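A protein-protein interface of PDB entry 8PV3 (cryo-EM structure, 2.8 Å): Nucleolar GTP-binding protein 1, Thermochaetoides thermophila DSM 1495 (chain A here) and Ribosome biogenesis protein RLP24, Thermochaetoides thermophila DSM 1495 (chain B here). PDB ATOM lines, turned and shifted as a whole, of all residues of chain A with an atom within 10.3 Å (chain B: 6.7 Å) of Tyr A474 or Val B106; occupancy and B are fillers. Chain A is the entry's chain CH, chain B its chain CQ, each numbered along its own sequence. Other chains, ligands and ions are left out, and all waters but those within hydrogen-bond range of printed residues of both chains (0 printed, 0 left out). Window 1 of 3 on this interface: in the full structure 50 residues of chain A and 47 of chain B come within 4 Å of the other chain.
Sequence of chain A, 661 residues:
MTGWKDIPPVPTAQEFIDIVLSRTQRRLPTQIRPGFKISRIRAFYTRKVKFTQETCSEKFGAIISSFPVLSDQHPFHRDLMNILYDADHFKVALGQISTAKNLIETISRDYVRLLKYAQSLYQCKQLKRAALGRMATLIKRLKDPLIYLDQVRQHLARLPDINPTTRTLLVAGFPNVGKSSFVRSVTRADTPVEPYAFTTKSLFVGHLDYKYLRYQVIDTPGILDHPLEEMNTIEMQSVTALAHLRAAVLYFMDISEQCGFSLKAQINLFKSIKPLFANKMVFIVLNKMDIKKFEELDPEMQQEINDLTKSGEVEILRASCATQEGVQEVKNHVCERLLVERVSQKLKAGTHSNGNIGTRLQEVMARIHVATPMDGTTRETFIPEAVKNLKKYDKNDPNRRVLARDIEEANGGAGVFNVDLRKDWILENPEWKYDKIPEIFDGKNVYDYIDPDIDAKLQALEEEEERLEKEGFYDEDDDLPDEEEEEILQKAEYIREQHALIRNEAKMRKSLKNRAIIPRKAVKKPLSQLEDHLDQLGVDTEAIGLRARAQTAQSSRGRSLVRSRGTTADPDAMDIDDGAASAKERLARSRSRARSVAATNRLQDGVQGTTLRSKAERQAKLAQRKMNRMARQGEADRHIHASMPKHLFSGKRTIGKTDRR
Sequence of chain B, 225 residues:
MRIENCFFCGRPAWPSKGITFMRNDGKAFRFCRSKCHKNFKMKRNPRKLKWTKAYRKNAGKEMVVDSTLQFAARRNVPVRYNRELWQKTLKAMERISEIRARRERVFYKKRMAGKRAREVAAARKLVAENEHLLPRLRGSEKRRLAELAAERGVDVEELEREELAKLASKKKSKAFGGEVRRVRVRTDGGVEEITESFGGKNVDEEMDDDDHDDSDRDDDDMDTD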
ATOM      1  N   LEU A 461     -25.621  21.225  20.482  1.00  0.00           N
ATOM      2  CA  LEU A 461     -24.495  20.864  21.339  1.00  0.00           C
ATOM      3  C   LEU A 461     -24.939  20.002  22.514  1.00  0.00           C
ATOM      4  O   LEU A 461     -24.240  19.056  22.894  1.00  0.00           O
ATOM      5  CB  LEU A 461     -23.792  22.128  21.833  1.00  0.00           C
ATOM      6  CG  LEU A 461     -22.565  21.943  22.727  1.00  0.00           C
ATOM      7  CD1 LEU A 461     -21.476  21.187  21.992  1.00  0.00           C
ATOM      8  CD2 LEU A 461     -22.054  23.287  23.211  1.00  0.00           C
ATOM      9  N   GLU A 462     -26.099  20.306  23.101  1.00  0.00           N
ATOM     10  CA  GLU A 462     -26.595  19.496  24.212  1.00  0.00           C
ATOM     11  C   GLU A 462     -27.019  18.105  23.751  1.00  0.00           C
ATOM     12  O   GLU A 462     -26.811  17.123  24.474  1.00  0.00           O
ATOM     13  CB  GLU A 462     -27.751  20.207  24.917  1.00  0.00           C
ATOM     14  CG  GLU A 462     -27.348  21.480  25.646  1.00  0.00           C
ATOM     15  CD  GLU A 462     -26.724  21.212  27.004  1.00  0.00           C
ATOM     16  OE1 GLU A 462     -26.721  20.043  27.447  1.00  0.00           O
ATOM     17  OE2 GLU A 462     -26.231  22.172  27.632  1.00  0.00           O
ATOM     18  N   GLU A 463     -27.615  17.997  22.559  1.00  0.00           N
ATOM     19  CA  GLU A 463     -27.936  16.680  22.013  1.00  0.00           C
ATOM     20  C   GLU A 463     -26.672  15.877  21.733  1.00  0.00           C
ATOM     21  O   GLU A 463     -26.627  14.666  21.983  1.00  0.00           O
ATOM     22  CB  GLU A 463     -28.780  16.814  20.744  1.00  0.00           C
ATOM     23  CG  GLU A 463     -30.169  17.388  20.967  1.00  0.00           C
ATOM     24  CD  GLU A 463     -31.059  16.469  21.780  1.00  0.00           C
ATOM     25  OE1 GLU A 463     -30.898  15.235  21.676  1.00  0.00           O
ATOM     26  OE2 GLU A 463     -31.922  16.981  22.522  1.00  0.00           O
ATOM     27  N   GLU A 464     -25.630  16.538  21.220  1.00  0.00           N
ATOM     28  CA  GLU A 464     -24.355  15.858  21.005  1.00  0.00           C
ATOM     29  C   GLU A 464     -23.737  15.406  22.323  1.00  0.00           C
ATOM     30  O   GLU A 464     -23.196  14.298  22.414  1.00  0.00           O
ATOM     31  CB  GLU A 464     -23.399  16.773  20.243  1.00  0.00           C
ATOM     32  CG  GLU A 464     -22.026  16.177  19.991  1.00  0.00           C
ATOM     33  CD  GLU A 464     -21.087  17.151  19.311  1.00  0.00           C
ATOM     34  OE1 GLU A 464     -21.471  18.327  19.148  1.00  0.00           O
ATOM     35  OE2 GLU A 464     -19.967  16.744  18.939  1.00  0.00           O
ATOM     36  N   GLU A 465     -23.824  16.244  23.360  1.00  0.00           N
ATOM     37  CA  GLU A 465     -23.299  15.880  24.674  1.00  0.00           C
ATOM     38  C   GLU A 465     -24.055  14.695  25.265  1.00  0.00           C
ATOM     39  O   GLU A 465     -23.455  13.798  25.870  1.00  0.00           O
ATOM     40  CB  GLU A 465     -23.369  17.086  25.613  1.00  0.00           C
ATOM     41  CG  GLU A 465     -22.781  16.850  26.998  1.00  0.00           C
ATOM     42  CD  GLU A 465     -21.265  16.932  27.032  1.00  0.00           C
ATOM     43  OE1 GLU A 465     -20.651  17.249  25.992  1.00  0.00           O
ATOM     44  OE2 GLU A 465     -20.683  16.677  28.107  1.00  0.00           O
ATOM     45  N   GLU A 466     -25.379  14.676  25.095  1.00  0.00           N
ATOM     46  CA  GLU A 466     -26.179  13.557  25.581  1.00  0.00           C
ATOM     47  C   GLU A 466     -25.853  12.278  24.817  1.00  0.00           C
ATOM     48  O   GLU A 466     -25.800  11.187  25.399  1.00  0.00           O
ATOM     49  CB  GLU A 466     -27.667  13.897  25.471  1.00  0.00           C
ATOM     50  CG  GLU A 466     -28.613  12.824  25.992  1.00  0.00           C
ATOM     51  CD  GLU A 466     -28.492  12.592  27.489  1.00  0.00           C
ATOM     52  OE1 GLU A 466     -28.080  13.522  28.216  1.00  0.00           O
ATOM     53  OE2 GLU A 466     -28.811  11.472  27.941  1.00  0.00           O
ATOM     54  N   ARG A 467     -25.620  12.399  23.507  1.00  0.00           N
ATOM     55  CA  ARG A 467     -25.224  11.249  22.700  1.00  0.00           C
ATOM     56  C   ARG A 467     -23.873  10.699  23.145  1.00  0.00           C
ATOM     57  O   ARG A 467     -23.680   9.480  23.223  1.00  0.00           O
ATOM     58  CB  ARG A 467     -25.187  11.644  21.225  1.00  0.00           C
ATOM     59  CG  ARG A 467     -24.762  10.531  20.289  1.00  0.00           C
ATOM     60  CD  ARG A 467     -25.190  10.828  18.852  1.00  0.00           C
ATOM     61  NE  ARG A 467     -24.401  11.869  18.194  1.00  0.00           N
ATOM     62  CZ  ARG A 467     -23.100  11.813  17.927  1.00  0.00           C
ATOM     63  NH1 ARG A 467     -22.386  10.719  18.146  1.00  0.00           N
ATOM     64  NH2 ARG A 467     -22.505  12.875  17.392  1.00  0.00           N
ATOM     65  N   LEU A 468     -22.925  11.589  23.448  1.00  0.00           N
ATOM     66  CA  LEU A 468     -21.615  11.144  23.915  1.00  0.00           C
ATOM     67  C   LEU A 468     -21.698  10.514  25.302  1.00  0.00           C
ATOM     68  O   LEU A 468     -20.971   9.559  25.600  1.00  0.00           O
ATOM     69  CB  LEU A 468     -20.624  12.309  23.902  1.00  0.00           C
ATOM     70  CG  LEU A 468     -20.275  12.939  22.549  1.00  0.00           C
ATOM     71  CD1 LEU A 468     -18.974  13.710  22.626  1.00  0.00           C
ATOM     72  CD2 LEU A 468     -20.195  11.889  21.450  1.00  0.00           C
ATOM     73  N   GLU A 469     -22.577  11.032  26.165  1.00  0.00           N
ATOM     74  CA  GLU A 469     -22.775  10.405  27.470  1.00  0.00           C
ATOM     75  C   GLU A 469     -23.424   9.030  27.334  1.00  0.00           C
ATOM     76  O   GLU A 469     -23.141   8.124  28.126  1.00  0.00           O
ATOM     77  CB  GLU A 469     -23.614  11.305  28.377  1.00  0.00           C
ATOM     78  CG  GLU A 469     -22.833  12.446  29.004  1.00  0.00           C
ATOM     79  CD  GLU A 469     -23.725  13.434  29.726  1.00  0.00           C
ATOM     80  OE1 GLU A 469     -24.959  13.364  29.549  1.00  0.00           O
ATOM     81  OE2 GLU A 469     -23.193  14.279  30.476  1.00  0.00           O
ATOM     82  N   LYS A 470     -24.312   8.863  26.348  1.00  0.00           N
ATOM     83  CA  LYS A 470     -24.846   7.534  26.058  1.00  0.00           C
ATOM     84  C   LYS A 470     -23.757   6.596  25.550  1.00  0.00           C
ATOM     85  O   LYS A 470     -23.701   5.428  25.951  1.00  0.00           O
ATOM     86  CB  LYS A 470     -25.978   7.621  25.035  1.00  0.00           C
ATOM     87  CG  LYS A 470     -27.275   8.207  25.556  1.00  0.00           C
ATOM     88  CD  LYS A 470     -28.176   8.616  24.401  1.00  0.00           C
ATOM     89  CE  LYS A 470     -29.381   9.403  24.882  1.00  0.00           C
ATOM     90  NZ  LYS A 470     -30.184   9.931  23.744  1.00  0.00           N
ATOM     91  N   GLU A 471     -22.883   7.089  24.673  1.00  0.00           N
ATOM     92  CA  GLU A 471     -21.848   6.254  24.074  1.00  0.00           C
ATOM     93  C   GLU A 471     -20.630   6.070  24.970  1.00  0.00           C
ATOM     94  O   GLU A 471     -19.722   5.319  24.594  1.00  0.00           O
ATOM     95  CB  GLU A 471     -21.413   6.839  22.729  1.00  0.00           C
ATOM     96  CG  GLU A 471     -22.493   6.815  21.661  1.00  0.00           C
ATOM     97  CD  GLU A 471     -22.864   5.408  21.232  1.00  0.00           C
ATOM     98  OE1 GLU A 471     -21.982   4.524  21.251  1.00  0.00           O
ATOM     99  OE2 GLU A 471     -24.040   5.185  20.879  1.00  0.00           O
ATOM    100  N   GLY A 472     -20.577   6.725  26.127  1.00  0.00           N
ATOM    101  CA  GLY A 472     -19.451   6.535  27.019  1.00  0.00           C
ATOM    102  C   GLY A 472     -18.193   7.266  26.619  1.00  0.00           C
ATOM    103  O   GLY A 472     -17.093   6.761  26.861  1.00  0.00           O
ATOM    104  N   PHE A 473     -18.325   8.438  25.994  1.00  0.00           N
ATOM    105  CA  PHE A 473     -17.155   9.224  25.616  1.00  0.00           C
ATOM    106  C   PHE A 473     -16.420   9.744  26.844  1.00  0.00           C
ATOM    107  O   PHE A 473     -15.188   9.848  26.843  1.00  0.00           O
ATOM    108  CB  PHE A 473     -17.584  10.383  24.719  1.00  0.00           C
ATOM    109  CG  PHE A 473     -16.442  11.158  24.130  1.00  0.00           C
ATOM    110  CD1 PHE A 473     -16.209  12.470  24.510  1.00  0.00           C
ATOM    111  CD2 PHE A 473     -15.618  10.585  23.178  1.00  0.00           C
ATOM    112  CE1 PHE A 473     -15.170  13.191  23.964  1.00  0.00           C
ATOM    113  CE2 PHE A 473     -14.574  11.301  22.625  1.00  0.00           C
ATOM    114  CZ  PHE A 473     -14.352  12.605  23.018  1.00  0.00           C
ATOM    115  N   TYR A 474     -17.159  10.072  27.901  1.00  0.00           N
ATOM    116  CA  TYR A 474     -16.589  10.601  29.132  1.00  0.00           C
ATOM    117  C   TYR A 474     -16.360   9.528  30.189  1.00  0.00           C
ATOM    118  O   TYR A 474     -16.035   9.865  31.331  1.00  0.00           O
ATOM    119  CB  TYR A 474     -17.489  11.699  29.700  1.00  0.00           C
ATOM    120  CG  TYR A 474     -17.738  12.849  28.751  1.00  0.00           C
ATOM    121  CD1 TYR A 474     -16.867  13.927  28.696  1.00  0.00           C
ATOM    122  CD2 TYR A 474     -18.848  12.859  27.917  1.00  0.00           C
ATOM    123  CE1 TYR A 474     -17.089  14.980  27.834  1.00  0.00           C
ATOM    124  CE2 TYR A 474     -19.079  13.909  27.050  1.00  0.00           C
ATOM    125  CZ  TYR A 474     -18.196  14.967  27.014  1.00  0.00           C
ATOM    126  OH  TYR A 474     -18.419  16.016  26.154  1.00  0.00           O
ATOM    127  N   ASP A 475     -16.528   8.256  29.840  1.00  0.00           N
ATOM    128  CA  ASP A 475     -16.359   7.171  30.799  1.00  0.00           C
ATOM    129  C   ASP A 475     -14.877   6.957  31.084  1.00  0.00           C
ATOM    130  O   ASP A 475     -14.071   6.841  30.156  1.00  0.00           O
ATOM    131  CB  ASP A 475     -16.996   5.889  30.269  1.00  0.00           C
ATOM    132  CG  ASP A 475     -18.507   5.898  30.386  1.00  0.00           C
ATOM    133  OD1 ASP A 475     -19.075   6.974  30.670  1.00  0.00           O
ATOM    134  OD2 ASP A 475     -19.126   4.831  30.195  1.00  0.00           O
ATOM    135  N   GLU A 476     -14.524   6.901  32.364  1.00  0.00           N
ATOM    136  CA  GLU A 476     -13.151   6.684  32.796  1.00  0.00           C
ATOM    137  C   GLU A 476     -12.989   5.246  33.270  1.00  0.00           C
ATOM    138  O   GLU A 476     -13.960   4.619  33.708  1.00  0.00           O
ATOM    139  CB  GLU A 476     -12.770   7.655  33.914  1.00  0.00           C
ATOM    140  CG  GLU A 476     -12.938   9.121  33.549  1.00  0.00           C
ATOM    141  CD  GLU A 476     -12.516  10.051  34.670  1.00  0.00           C
ATOM    142  OE1 GLU A 476     -12.061   9.552  35.721  1.00  0.00           O
ATOM    143  OE2 GLU A 476     -12.640  11.282  34.500  1.00  0.00           O
ATOM    144  N   ASP A 477     -11.768   4.731  33.181  1.00  0.00           N
ATOM    145  CA  ASP A 477     -11.482   3.367  33.608  1.00  0.00           C
ATOM    146  C   ASP A 477     -11.421   3.267  35.129  1.00  0.00           C
ATOM    147  O   ASP A 477     -11.365   4.281  35.826  1.00  0.00           O
ATOM    148  CB  ASP A 477     -10.167   2.879  32.996  1.00  0.00           C
ATOM    149  CG  ASP A 477     -10.256   2.704  31.494  1.00  0.00           C
ATOM    150  OD1 ASP A 477     -11.362   2.413  30.992  1.00  0.00           O
ATOM    151  OD2 ASP A 477      -9.219   2.856  30.815  1.00  0.00           O
ATOM    152  N   ILE B  99     -18.217  22.305  28.902  1.00  0.00           N
ATOM    153  CA  ILE B  99     -18.100  21.214  27.933  1.00  0.00           C
ATOM    154  C   ILE B  99     -16.703  21.186  27.314  1.00  0.00           C
ATOM    155  O   ILE B  99     -16.122  20.111  27.096  1.00  0.00           O
ATOM    156  CB  ILE B  99     -19.195  21.331  26.857  1.00  0.00           C
ATOM    157  CG1 ILE B  99     -20.580  21.279  27.495  1.00  0.00           C
ATOM    158  CG2 ILE B  99     -19.081  20.211  25.845  1.00  0.00           C
ATOM    159  CD1 ILE B  99     -21.698  21.495  26.509  1.00  0.00           C
ATOM    160  N   ALA B 101     -13.922  22.157  28.783  1.00  0.00           N
ATOM    161  CA  ALA B 101     -13.002  21.601  29.771  1.00  0.00           C
ATOM    162  C   ALA B 101     -13.073  20.078  29.811  1.00  0.00           C
ATOM    163  O   ALA B 101     -12.034  19.399  29.842  1.00  0.00           O
ATOM    164  CB  ALA B 101     -13.299  22.188  31.150  1.00  0.00           C
ATOM    165  N   ARG B 102     -14.292  19.526  29.788  1.00  0.00           N
ATOM    166  CA  ARG B 102     -14.439  18.068  29.831  1.00  0.00           C
ATOM    167  C   ARG B 102     -13.827  17.405  28.597  1.00  0.00           C
ATOM    168  O   ARG B 102     -13.085  16.414  28.705  1.00  0.00           O
ATOM    169  CB  ARG B 102     -15.916  17.696  29.967  1.00  0.00           C
ATOM    170  CG  ARG B 102     -16.446  17.805  31.384  1.00  0.00           C
ATOM    171  CD  ARG B 102     -17.271  16.588  31.765  1.00  0.00           C
ATOM    172  NE  ARG B 102     -18.448  16.433  30.920  1.00  0.00           N
ATOM    173  CZ  ARG B 102     -19.250  15.378  30.940  1.00  0.00           C
ATOM    174  NH1 ARG B 102     -19.026  14.355  31.747  1.00  0.00           N
ATOM    175  NH2 ARG B 102     -20.305  15.350  30.131  1.00  0.00           N
ATOM    176  N   ARG B 103     -14.101  17.959  27.414  1.00  0.00           N
ATOM    177  CA  ARG B 103     -13.576  17.360  26.191  1.00  0.00           C
ATOM    178  C   ARG B 103     -12.063  17.539  26.082  1.00  0.00           C
ATOM    179  O   ARG B 103     -11.374  16.681  25.517  1.00  0.00           O
ATOM    180  CB  ARG B 103     -14.292  17.945  24.977  1.00  0.00           C
ATOM    181  CG  ARG B 103     -15.775  17.620  24.958  1.00  0.00           C
ATOM    182  CD  ARG B 103     -16.425  18.004  23.646  1.00  0.00           C
ATOM    183  NE  ARG B 103     -17.843  17.670  23.626  1.00  0.00           N
ATOM    184  CZ  ARG B 103     -18.647  17.890  22.596  1.00  0.00           C
ATOM    185  NH1 ARG B 103     -18.204  18.442  21.479  1.00  0.00           N
ATOM    186  NH2 ARG B 103     -19.929  17.551  22.690  1.00  0.00           N
ATOM    187  N   GLU B 104     -11.527  18.631  26.638  1.00  0.00           N
ATOM    188  CA  GLU B 104     -10.080  18.811  26.673  1.00  0.00           C
ATOM    189  C   GLU B 104      -9.410  17.765  27.555  1.00  0.00           C
ATOM    190  O   GLU B 104      -8.336  17.249  27.213  1.00  0.00           O
ATOM    191  CB  GLU B 104      -9.743  20.220  27.160  1.00  0.00           C
ATOM    192  CG  GLU B 104      -8.324  20.665  26.852  1.00  0.00           C
ATOM    193  CD  GLU B 104      -7.346  20.311  27.958  1.00  0.00           C
ATOM    194  OE1 GLU B 104      -7.721  20.429  29.144  1.00  0.00           O
ATOM    195  OE2 GLU B 104      -6.206  19.911  27.642  1.00  0.00           O
ATOM    196  N   ARG B 105     -10.020  17.450  28.703  1.00  0.00           N
ATOM    197  CA  ARG B 105      -9.462  16.403  29.556  1.00  0.00           C
ATOM    198  C   ARG B 105      -9.496  15.044  28.860  1.00  0.00           C
ATOM    199  O   ARG B 105      -8.543  14.257  28.971  1.00  0.00           O
ATOM    200  CB  ARG B 105     -10.209  16.342  30.886  1.00  0.00           C
ATOM    201  CG  ARG B 105      -9.454  15.581  31.960  1.00  0.00           C
ATOM    202  CD  ARG B 105     -10.329  15.289  33.165  1.00  0.00           C
ATOM    203  NE  ARG B 105      -9.745  14.264  34.022  1.00  0.00           N
ATOM    204  CZ  ARG B 105      -8.802  14.489  34.928  1.00  0.00           C
ATOM    205  NH1 ARG B 105      -8.315  15.702  35.134  1.00  0.00           N
ATOM    206  NH2 ARG B 105      -8.339  13.472  35.648  1.00  0.00           N
ATOM    207  N   VAL B 106     -10.581  14.763  28.129  1.00  0.00           N
ATOM    208  CA  VAL B 106     -10.660  13.521  27.356  1.00  0.00           C
ATOM    209  C   VAL B 106      -9.558  13.470  26.296  1.00  0.00           C
ATOM    210  O   VAL B 106      -8.911  12.431  26.096  1.00  0.00           O
ATOM    211  CB  VAL B 106     -12.059  13.371  26.731  1.00  0.00           C
ATOM    212  CG1 VAL B 106     -12.102  12.187  25.783  1.00  0.00           C
ATOM    213  CG2 VAL B 106     -13.109  13.214  27.813  1.00  0.00           C
ATOM    214  N   PHE B 107      -9.325  14.599  25.615  1.00  0.00           N
ATOM    215  CA  PHE B 107      -8.274  14.685  24.601  1.00  0.00           C
ATOM    216  C   PHE B 107      -6.896  14.412  25.196  1.00  0.00           C
ATOM    217  O   PHE B 107      -6.089  13.674  24.611  1.00  0.00           O
ATOM    218  CB  PHE B 107      -8.321  16.073  23.955  1.00  0.00           C
ATOM    219  CG  PHE B 107      -7.383  16.252  22.794  1.00  0.00           C
ATOM    220  CD1 PHE B 107      -7.781  15.917  21.514  1.00  0.00           C
ATOM    221  CD2 PHE B 107      -6.120  16.794  22.976  1.00  0.00           C
ATOM    222  CE1 PHE B 107      -6.928  16.092  20.442  1.00  0.00           C
ATOM    223  CE2 PHE B 107      -5.264  16.969  21.908  1.00  0.00           C
ATOM    224  CZ  PHE B 107      -5.669  16.620  20.642  1.00  0.00           C
ATOM    225  N   TYR B 108      -6.614  14.985  26.370  1.00  0.00           N
ATOM    226  CA  TYR B 108      -5.308  14.788  26.993  1.00  0.00           C
ATOM    227  C   TYR B 108      -5.112  13.341  27.437  1.00  0.00           C
ATOM    228  O   TYR B 108      -4.014  12.784  27.298  1.00  0.00           O
ATOM    229  CB  TYR B 108      -5.129  15.741  28.172  1.00  0.00           C
ATOM    230  CG  TYR B 108      -3.702  15.811  28.662  1.00  0.00           C
ATOM    231  CD1 TYR B 108      -2.735  16.495  27.942  1.00  0.00           C
ATOM    232  CD2 TYR B 108      -3.319  15.186  29.838  1.00  0.00           C
ATOM    233  CE1 TYR B 108      -1.431  16.558  28.382  1.00  0.00           C
ATOM    234  CE2 TYR B 108      -2.016  15.245  30.288  1.00  0.00           C
ATOM    235  CZ  TYR B 108      -1.077  15.932  29.555  1.00  0.00           C
ATOM    236  OH  TYR B 108       0.223  15.996  29.997  1.00  0.00           O
ATOM    237  N   LYS B 109      -6.163  12.713  27.974  1.00  0.00           N
ATOM    238  CA  LYS B 109      -6.045  11.304  28.349  1.00  0.00           C
ATOM    239  C   LYS B 109      -5.832  10.408  27.131  1.00  0.00           C
ATOM    240  O   LYS B 109      -5.072   9.428  27.200  1.00  0.00           O
ATOM    241  CB  LYS B 109      -7.281  10.863  29.131  1.00  0.00           C
ATOM    242  CG  LYS B 109      -7.401  11.521  30.493  1.00  0.00           C
ATOM    243  CD  LYS B 109      -8.683  11.121  31.191  1.00  0.00           C
ATOM    244  CE  LYS B 109      -8.619   9.677  31.651  1.00  0.00           C
ATOM    245  NZ  LYS B 109      -7.618   9.496  32.737  1.00  0.00           N
ATOM    246  N   LYS B 110      -6.484  10.729  26.009  1.00  0.00           N
ATOM    247  CA  LYS B 110      -6.245   9.973  24.783  1.00  0.00           C
ATOM    248  C   LYS B 110      -4.820  10.167  24.277  1.00  0.00           C
ATOM    249  O   LYS B 110      -4.254   9.266  23.648  1.00  0.00           O
ATOM    250  CB  LYS B 110      -7.255  10.369  23.710  1.00  0.00           C
ATOM    251  CG  LYS B 110      -8.628   9.758  23.904  1.00  0.00           C
ATOM    252  CD  LYS B 110      -9.544  10.088  22.740  1.00  0.00           C
ATOM    253  CE  LYS B 110     -10.877   9.375  22.869  1.00  0.00           C
ATOM    254  NZ  LYS B 110     -11.797   9.722  21.751  1.00  0.00           N
ATOM    255  N   ARG B 111      -4.229  11.338  24.531  1.00  0.00           N
ATOM    256  CA  ARG B 111      -2.811  11.507  24.215  1.00  0.00           C
ATOM    257  C   ARG B 111      -1.914  10.693  25.145  1.00  0.00           C
ATOM    258  O   ARG B 111      -0.870  10.192  24.711  1.00  0.00           O
ATOM    259  CB  ARG B 111      -2.410  12.981  24.278  1.00  0.00           C
ATOM    260  CG  ARG B 111      -3.095  13.864  23.260  1.00  0.00           C
ATOM    261  CD  ARG B 111      -2.181  14.985  22.789  1.00  0.00           C
ATOM    262  NE  ARG B 111      -1.832  15.920  23.852  1.00  0.00           N
ATOM    263  CZ  ARG B 111      -0.602  16.120  24.304  1.00  0.00           C
ATOM    264  NH1 ARG B 111       0.430  15.454  23.816  1.00  0.00           N
ATOM    265  NH2 ARG B 111      -0.400  17.017  25.263  1.00  0.00           N
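The guanidinium group (NH2) of Arg B102 is in salt-bridge range of the side-chain carboxylate (OE2) of Glu A465 (2.4 Å).
NH2 of Arg B102 is in salt-bridge range of OE2 of Glu A469, 3.1 Å away.
The side-chain carboxylate (OE2) of Glu A464 lies within salt-bridge range of the guanidinium group (NH1) of Arg B103, 3.5 Å away.
The guanidinium group of Arg B103 is in salt-bridge range of the side-chain carboxylate of Glu A465 (3.4 Å).
The guanidinium group of Arg B103 sits at hydrogen-bond distance from the side-chain hydroxyl of Tyr A474 (3.1 Å).
The side-chain carboxylate of Glu A465 lies within hydrogen-bond range of the side-chain hydroxyl of Tyr A474 (2.6 Å).
O of Leu A468 sits at hydrogen-bond distance from N of Phe A473, 2.9 Å away.
Among the printed residues, merely in contact across the chains: Leu A461 with Ile B99 (3.8 Å), Glu A465 with Ile B99 (3.4 Å), Leu A468 with Arg B103 (3.96 Å), Phe A473 with Val B106 (3.6 Å), Phe A473 with Lys B110 (3.3 Å), Tyr A474 with Arg B102 (3.6 Å) and Tyr A474 with Val B106 (3.9 Å).
Printed residues of chain B within 4 Å of Glu A464: Arg B103 (3.5 Å).
Glu A466 touches none of the printed residues of chain B.
Of the printed residues of chain A, Ile B99 touches Leu A461 (3.8 Å) and Glu A465 (3.4 Å).
Arg B102 touches just these residues of chain A: Glu A465, Glu A469 and Tyr A474.
Of the printed residues of chain A, Arg B103 touches Glu A464, Glu A465, Leu A468 and Tyr A474.
Lys B109 touches none of the printed residues of chain A.
Lys B110 touches just one residue of chain A: Phe A473.
Of the 17 printed residues of chain A, 7 touch a printed residue of chain B.
Printed residues of chain B that touch a printed residue of chain A: Ile B99, Arg B102, Arg B103, Val B106 and Lys B110.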
